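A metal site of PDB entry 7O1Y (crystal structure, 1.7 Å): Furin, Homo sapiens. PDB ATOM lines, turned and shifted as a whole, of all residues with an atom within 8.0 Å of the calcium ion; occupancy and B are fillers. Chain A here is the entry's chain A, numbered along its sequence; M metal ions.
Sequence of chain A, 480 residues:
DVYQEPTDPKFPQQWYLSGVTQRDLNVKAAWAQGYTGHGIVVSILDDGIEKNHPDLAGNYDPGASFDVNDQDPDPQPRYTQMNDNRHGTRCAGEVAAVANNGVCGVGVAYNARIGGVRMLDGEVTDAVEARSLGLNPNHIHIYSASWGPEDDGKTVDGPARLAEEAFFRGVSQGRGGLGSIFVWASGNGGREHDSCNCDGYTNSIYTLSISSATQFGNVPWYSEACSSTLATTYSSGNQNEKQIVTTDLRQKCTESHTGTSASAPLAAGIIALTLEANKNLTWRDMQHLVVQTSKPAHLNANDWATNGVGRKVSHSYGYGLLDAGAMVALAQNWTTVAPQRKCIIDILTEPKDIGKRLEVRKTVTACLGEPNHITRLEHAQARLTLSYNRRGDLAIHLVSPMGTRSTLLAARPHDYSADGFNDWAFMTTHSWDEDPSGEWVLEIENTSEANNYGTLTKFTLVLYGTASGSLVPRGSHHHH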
ATOM      1  N   PRO A   6      -3.662  19.171   6.873  1.00  0.00           N
ATOM      2  CA  PRO A   6      -4.908  18.413   7.070  1.00  0.00           C
ATOM      3  C   PRO A   6      -4.899  17.503   8.289  1.00  0.00           C
ATOM      4  O   PRO A   6      -3.876  16.926   8.651  1.00  0.00           O
ATOM      5  CB  PRO A   6      -5.030  17.590   5.781  1.00  0.00           C
ATOM      6  CG  PRO A   6      -4.353  18.416   4.768  1.00  0.00           C
ATOM      7  CD  PRO A   6      -3.175  19.041   5.491  1.00  0.00           C
ATOM      8  N   THR A   7      -6.065  17.359   8.894  1.00  0.00           N
ATOM      9  CA  THR A   7      -6.249  16.552  10.089  1.00  0.00           C
ATOM     10  C   THR A   7      -6.936  15.219   9.810  1.00  0.00           C
ATOM     11  O   THR A   7      -7.172  14.453  10.738  1.00  0.00           O
ATOM     12  CB  THR A   7      -7.075  17.330  11.113  1.00  0.00           C
ATOM     13  OG1 THR A   7      -8.378  17.599  10.565  1.00  0.00           O
ATOM     14  CG2 THR A   7      -6.386  18.647  11.469  1.00  0.00           C
ATOM     15  N   ASP A   8      -7.240  14.933   8.550  1.00  0.00           N
ATOM     16  CA  ASP A   8      -7.909  13.704   8.186  1.00  0.00           C
ATOM     17  C   ASP A   8      -7.133  12.494   8.687  1.00  0.00           C
ATOM     18  O   ASP A   8      -5.886  12.502   8.709  1.00  0.00           O
ATOM     19  CB  ASP A   8      -8.057  13.642   6.661  1.00  0.00           C
ATOM     20  CG  ASP A   8      -8.789  14.856   6.121  1.00  0.00           C
ATOM     21  OD1 ASP A   8      -8.223  15.968   6.218  1.00  0.00           O
ATOM     22  OD2 ASP A   8      -9.937  14.708   5.660  1.00  0.00           O
ATOM     23  N   PRO A   9      -7.842  11.427   9.085  1.00  0.00           N
ATOM     24  CA  PRO A   9      -7.189  10.316   9.780  1.00  0.00           C
ATOM     25  C   PRO A   9      -6.140   9.585   8.961  1.00  0.00           C
ATOM     26  O   PRO A   9      -5.196   9.051   9.546  1.00  0.00           O
ATOM     27  CB  PRO A   9      -8.366   9.383  10.140  1.00  0.00           C
ATOM     28  CG  PRO A   9      -9.478   9.781   9.249  1.00  0.00           C
ATOM     29  CD  PRO A   9      -9.303  11.254   9.020  1.00  0.00           C
ATOM     30  N   LYS A  10      -6.300   9.517   7.642  1.00  0.00           N
ATOM     31  CA  LYS A  10      -5.359   8.814   6.787  1.00  0.00           C
ATOM     32  C   LYS A  10      -4.369   9.745   6.094  1.00  0.00           C
ATOM     33  O   LYS A  10      -3.552   9.277   5.295  1.00  0.00           O
ATOM     34  CB  LYS A  10      -6.097   7.973   5.729  1.00  0.00           C
ATOM     35  CG  LYS A  10      -6.911   6.781   6.307  1.00  0.00           C
ATOM     36  CD  LYS A  10      -5.985   5.819   7.063  1.00  0.00           C
ATOM     37  CE  LYS A  10      -6.658   4.501   7.453  1.00  0.00           C
ATOM     38  N   PHE A  11      -4.426  11.063   6.368  1.00  0.00           N
ATOM     39  CA  PHE A  11      -3.466  11.952   5.701  1.00  0.00           C
ATOM     40  C   PHE A  11      -2.031  11.540   5.978  1.00  0.00           C
ATOM     41  O   PHE A  11      -1.197  11.626   5.055  1.00  0.00           O
ATOM     42  CB  PHE A  11      -3.685  13.405   6.110  1.00  0.00           C
ATOM     43  CG  PHE A  11      -2.689  14.345   5.495  1.00  0.00           C
ATOM     44  CD1 PHE A  11      -2.679  14.558   4.122  1.00  0.00           C
ATOM     45  CD2 PHE A  11      -1.775  15.021   6.280  1.00  0.00           C
ATOM     46  CE1 PHE A  11      -1.749  15.419   3.535  1.00  0.00           C
ATOM     47  CE2 PHE A  11      -0.872  15.880   5.716  1.00  0.00           C
ATOM     48  CZ  PHE A  11      -0.842  16.087   4.338  1.00  0.00           C
ATOM     49  N   GLN A  14      -0.762   9.172   3.460  1.00  0.00           N
ATOM     50  CA  GLN A  14      -0.627   9.683   2.081  1.00  0.00           C
ATOM     51  C   GLN A  14       0.793  10.229   1.908  1.00  0.00           C
ATOM     52  O   GLN A  14       1.043  11.429   1.787  1.00  0.00           O
ATOM     53  CB  GLN A  14      -1.697  10.741   1.805  1.00  0.00           C
ATOM     54  CG  GLN A  14      -3.111  10.117   1.859  1.00  0.00           C
ATOM     55  CD  GLN A  14      -4.245  11.097   1.531  1.00  0.00           C
ATOM     56  OE1 GLN A  14      -4.418  12.115   2.208  1.00  0.00           O
ATOM     57  NE2 GLN A  14      -5.030  10.780   0.496  1.00  0.00           N
ATOM     58  N   HIS A  53     -20.300   9.504  -1.571  1.00  0.00           N
ATOM     59  CA  HIS A  53     -19.214   9.126  -0.670  1.00  0.00           C
ATOM     60  C   HIS A  53     -18.992  10.251   0.340  1.00  0.00           C
ATOM     61  O   HIS A  53     -18.939  11.428  -0.058  1.00  0.00           O
ATOM     62  CB  HIS A  53     -17.930   8.845  -1.435  1.00  0.00           C
ATOM     63  CG  HIS A  53     -16.911   8.080  -0.651  1.00  0.00           C
ATOM     64  ND1 HIS A  53     -16.238   8.628   0.419  1.00  0.00           N
ATOM     65  CD2 HIS A  53     -16.453   6.814  -0.783  1.00  0.00           C
ATOM     66  CE1 HIS A  53     -15.410   7.733   0.925  1.00  0.00           C
ATOM     67  NE2 HIS A  53     -15.515   6.619   0.210  1.00  0.00           N
ATOM     68  N   PRO A  54     -18.874   9.959   1.638  1.00  0.00           N
ATOM     69  CA  PRO A  54     -18.668  11.033   2.618  1.00  0.00           C
ATOM     70  C   PRO A  54     -17.437  11.902   2.347  1.00  0.00           C
ATOM     71  O   PRO A  54     -17.391  13.039   2.845  1.00  0.00           O
ATOM     72  CB  PRO A  54     -18.525  10.292   3.952  1.00  0.00           C
ATOM     73  CG  PRO A  54     -18.971   8.915   3.712  1.00  0.00           C
ATOM     74  CD  PRO A  54     -18.826   8.620   2.267  1.00  0.00           C
ATOM     75  N   ASP A  55     -16.430  11.429   1.607  1.00  0.00           N
ATOM     76  CA  ASP A  55     -15.263  12.245   1.307  1.00  0.00           C
ATOM     77  C   ASP A  55     -15.320  12.863  -0.083  1.00  0.00           C
ATOM     78  O   ASP A  55     -14.362  13.548  -0.478  1.00  0.00           O
ATOM     79  CB  ASP A  55     -13.977  11.433   1.472  1.00  0.00           C
ATOM     80  CG  ASP A  55     -12.915  12.150   2.318  1.00  0.00           C
ATOM     81  OD1 ASP A  55     -13.270  13.059   3.114  1.00  0.00           O
ATOM     82  OD2 ASP A  55     -11.722  11.801   2.172  1.00  0.00           O
ATOM     83  N   LEU A  56     -16.393  12.626  -0.851  1.00  0.00           N
ATOM     84  CA  LEU A  56     -16.583  13.241  -2.159  1.00  0.00           C
ATOM     85  C   LEU A  56     -17.799  14.169  -2.239  1.00  0.00           C
ATOM     86  O   LEU A  56     -17.760  15.135  -3.005  1.00  0.00           O
ATOM     87  CB  LEU A  56     -16.763  12.162  -3.249  1.00  0.00           C
ATOM     88  CG  LEU A  56     -15.589  11.209  -3.462  1.00  0.00           C
ATOM     89  CD1 LEU A  56     -15.949  10.223  -4.552  1.00  0.00           C
ATOM     90  CD2 LEU A  56     -14.301  11.962  -3.797  1.00  0.00           C
ATOM     91  N   ALA A  96      -9.710  15.147  -5.354  1.00  0.00           N
ATOM     92  CA  ALA A  96     -10.519  16.140  -4.649  1.00  0.00           C
ATOM     93  C   ALA A  96     -11.269  15.568  -3.453  1.00  0.00           C
ATOM     94  O   ALA A  96     -12.355  16.059  -3.133  1.00  0.00           O
ATOM     95  CB  ALA A  96     -11.497  16.788  -5.637  1.00  0.00           C
ATOM     96  N   ALA A  97     -10.724  14.566  -2.778  1.00  0.00           N
ATOM     97  CA  ALA A  97     -11.322  14.182  -1.508  1.00  0.00           C
ATOM     98  C   ALA A  97     -11.337  15.355  -0.545  1.00  0.00           C
ATOM     99  O   ALA A  97     -10.373  16.143  -0.483  1.00  0.00           O
ATOM    100  CB  ALA A  97     -10.578  13.009  -0.885  1.00  0.00           C
ATOM    101  N   VAL A  98     -12.420  15.462   0.228  1.00  0.00           N
ATOM    102  CA  VAL A  98     -12.639  16.594   1.116  1.00  0.00           C
ATOM    103  C   VAL A  98     -11.628  16.554   2.250  1.00  0.00           C
ATOM    104  O   VAL A  98     -11.239  15.479   2.727  1.00  0.00           O
ATOM    105  CB  VAL A  98     -14.078  16.564   1.643  1.00  0.00           C
ATOM    106  CG1 VAL A  98     -14.251  17.535   2.822  1.00  0.00           C
ATOM    107  CG2 VAL A  98     -15.064  16.877   0.517  1.00  0.00           C
ATOM    108  N   ALA A  99     -11.177  17.733   2.674  1.00  0.00           N
ATOM    109  CA  ALA A  99     -10.171  17.854   3.715  1.00  0.00           C
ATOM    110  C   ALA A  99     -10.773  18.264   5.046  1.00  0.00           C
ATOM    111  O   ALA A  99     -11.800  18.937   5.098  1.00  0.00           O
ATOM    112  CB  ALA A  99      -9.118  18.902   3.319  1.00  0.00           C
ATOM    113  N   ASN A 100     -10.099  17.856   6.119  1.00  0.00           N
ATOM    114  CA  ASN A 100     -10.412  18.302   7.489  1.00  0.00           C
ATOM    115  C   ASN A 100     -11.825  17.924   7.910  1.00  0.00           C
ATOM    116  O   ASN A 100     -12.497  18.669   8.642  1.00  0.00           O
ATOM    117  CB  ASN A 100     -10.178  19.804   7.611  1.00  0.00           C
ATOM    118  CG  ASN A 100      -8.720  20.187   7.379  1.00  0.00           C
ATOM    119  OD1 ASN A 100      -7.816  19.639   8.011  1.00  0.00           O
ATOM    120  ND2 ASN A 100      -8.490  21.094   6.443  1.00  0.00           N
ATOM    121  N   ASN A 101     -12.263  16.733   7.511  1.00  0.00           N
ATOM    122  CA  ASN A 101     -13.614  16.266   7.786  1.00  0.00           C
ATOM    123  C   ASN A 101     -13.654  14.927   8.519  1.00  0.00           C
ATOM    124  O   ASN A 101     -14.720  14.312   8.589  1.00  0.00           O
ATOM    125  CB  ASN A 101     -14.416  16.200   6.480  1.00  0.00           C
ATOM    126  CG  ASN A 101     -13.992  15.052   5.579  1.00  0.00           C
ATOM    127  OD1 ASN A 101     -12.861  14.565   5.675  1.00  0.00           O
ATOM    128  ND2 ASN A 101     -14.906  14.605   4.712  1.00  0.00           N
ATOM    129  N   GLY A 102     -12.542  14.467   9.083  1.00  0.00           N
ATOM    130  CA  GLY A 102     -12.508  13.230   9.825  1.00  0.00           C
ATOM    131  C   GLY A 102     -12.710  11.958   9.029  1.00  0.00           C
ATOM    132  O   GLY A 102     -12.912  10.899   9.631  1.00  0.00           O
ATOM    133  N   VAL A 103     -12.598  12.022   7.702  1.00  0.00           N
ATOM    134  CA  VAL A 103     -12.848  10.883   6.827  1.00  0.00           C
ATOM    135  C   VAL A 103     -11.641  10.671   5.906  1.00  0.00           C
ATOM    136  O   VAL A 103     -11.178  11.625   5.263  1.00  0.00           O
ATOM    137  CB  VAL A 103     -14.119  11.092   5.980  1.00  0.00           C
ATOM    138  CG1 VAL A 103     -14.310   9.959   4.979  1.00  0.00           C
ATOM    139  CG2 VAL A 103     -15.344  11.237   6.897  1.00  0.00           C
ATOM    140  N   CYS A 104     -11.104   9.447   5.901  1.00  0.00           N
ATOM    141  CA  CYS A 104     -10.062   8.985   4.967  1.00  0.00           C
ATOM    142  C   CYS A 104      -8.944  10.026   4.894  1.00  0.00           C
ATOM    143  O   CYS A 104      -8.467  10.466   5.958  1.00  0.00           O
ATOM    144  CB  CYS A 104     -10.741   8.649   3.636  1.00  0.00           C
ATOM    145  SG  CYS A 104      -9.802   7.565   2.494  1.00  0.00           S
ATOM    146  N   GLY A 105      -8.467  10.408   3.714  1.00  0.00           N
ATOM    147  CA  GLY A 105      -7.406  11.404   3.595  1.00  0.00           C
ATOM    148  C   GLY A 105      -7.906  12.642   2.872  1.00  0.00           C
ATOM    149  O   GLY A 105      -9.052  13.048   3.090  1.00  0.00           O
ATOM    150  N   VAL A 106      -7.077  13.253   2.015  1.00  0.00           N
ATOM    151  CA  VAL A 106      -7.460  14.440   1.260  1.00  0.00           C
ATOM    152  C   VAL A 106      -7.095  14.263  -0.210  1.00  0.00           C
ATOM    153  O   VAL A 106      -6.234  13.456  -0.577  1.00  0.00           O
ATOM    154  CB  VAL A 106      -6.806  15.729   1.814  1.00  0.00           C
ATOM    155  CG1 VAL A 106      -7.054  15.854   3.312  1.00  0.00           C
ATOM    156  CG2 VAL A 106      -5.318  15.757   1.499  1.00  0.00           C
ATOM    157  N   GLY A 107      -7.788  15.005  -1.050  1.00  0.00           N
ATOM    158  CA  GLY A 107      -7.342  15.156  -2.425  1.00  0.00           C
ATOM    159  C   GLY A 107      -6.195  16.134  -2.562  1.00  0.00           C
ATOM    160  O   GLY A 107      -5.966  17.001  -1.718  1.00  0.00           O
ATOM    161  N   TYR A 110      -8.069  19.678  -2.797  1.00  0.00           N
ATOM    162  CA  TYR A 110      -9.183  19.296  -1.947  1.00  0.00           C
ATOM    163  C   TYR A 110     -10.303  20.335  -1.895  1.00  0.00           C
ATOM    164  O   TYR A 110     -11.311  20.082  -1.212  1.00  0.00           O
ATOM    165  CB  TYR A 110      -8.697  18.974  -0.536  1.00  0.00           C
ATOM    166  CG  TYR A 110      -7.900  20.058   0.187  1.00  0.00           C
ATOM    167  CD1 TYR A 110      -8.494  21.240   0.635  1.00  0.00           C
ATOM    168  CD2 TYR A 110      -6.563  19.847   0.515  1.00  0.00           C
ATOM    169  CE1 TYR A 110      -7.770  22.199   1.326  1.00  0.00           C
ATOM    170  CE2 TYR A 110      -5.822  20.799   1.222  1.00  0.00           C
ATOM    171  CZ  TYR A 110      -6.437  21.973   1.621  1.00  0.00           C
ATOM    172  OH  TYR A 110      -5.716  22.914   2.338  1.00  0.00           O
ATOM    173  N   THR A 247     -10.425   7.346  -1.449  1.00  0.00           N
ATOM    174  CA  THR A 247     -11.818   6.933  -1.298  1.00  0.00           C
ATOM    175  C   THR A 247     -12.080   5.648  -2.068  1.00  0.00           C
ATOM    176  O   THR A 247     -11.537   5.431  -3.157  1.00  0.00           O
ATOM    177  CB  THR A 247     -12.720   8.049  -1.817  1.00  0.00           C
ATOM    178  OG1 THR A 247     -12.235   8.476  -3.104  1.00  0.00           O
ATOM    179  CG2 THR A 247     -12.676   9.245  -0.911  1.00  0.00           C
ATOM    180  N   CYS A 253     -12.539   3.534   2.617  1.00  0.00           N
ATOM    181  CA  CYS A 253     -11.214   4.146   2.399  1.00  0.00           C
ATOM    182  C   CYS A 253     -10.187   3.056   2.128  1.00  0.00           C
ATOM    183  O   CYS A 253     -10.038   2.139   2.953  1.00  0.00           O
ATOM    184  CB  CYS A 253     -10.827   4.963   3.635  1.00  0.00           C
ATOM    185  SG  CYS A 253      -9.297   5.906   3.569  1.00  0.00           S
HETATM  186 CA    CA M   1     -11.185  13.596   4.056  1.00  0.00          CA
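O of Pro 54 is in hydrogen-bond range of ND2 of Asn 101. The side-chain sulfur (SG) of Cys 104 is disulfide-bonded to the side-chain sulfur (SG) of Cys 253. N of Asp 55 sits at hydrogen-bond distance from ND1 of His 53. The backbone NH (N) of Asn 100 lies within hydrogen-bond range of the side-chain carboxylate (OD1) of Asp 8 (2.7 Å).
Within 4 Å of the calcium ion: Asp 8, Asp 55, Val 98, Asn 101, Val 103 and Gly 105. The nearest printed residue that does not touch the calcium ion is Cys 104 (4.3 Å).
O of Val 98 is bound to the calcium ion, at 2.3 Å. The backbone carbonyl oxygen (O) of Val 103 binds the calcium ion, 2.3 Å away. The calcium ion is bound by OD2 of Asp 8, at 2.3 Å. The side-chain carboxylate (OD1) of Asp 55 binds the calcium ion, at 2.4 Å. O of Gly 105 binds the calcium ion. The side-chain amide oxygen (OD1) of Asn 101 binds the calcium ion, 2.5 Å away. The side-chain carboxylate (OD2) of Asp 55 is bound to the calcium ion. The calcium ion has seven donor atoms within binding distance.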
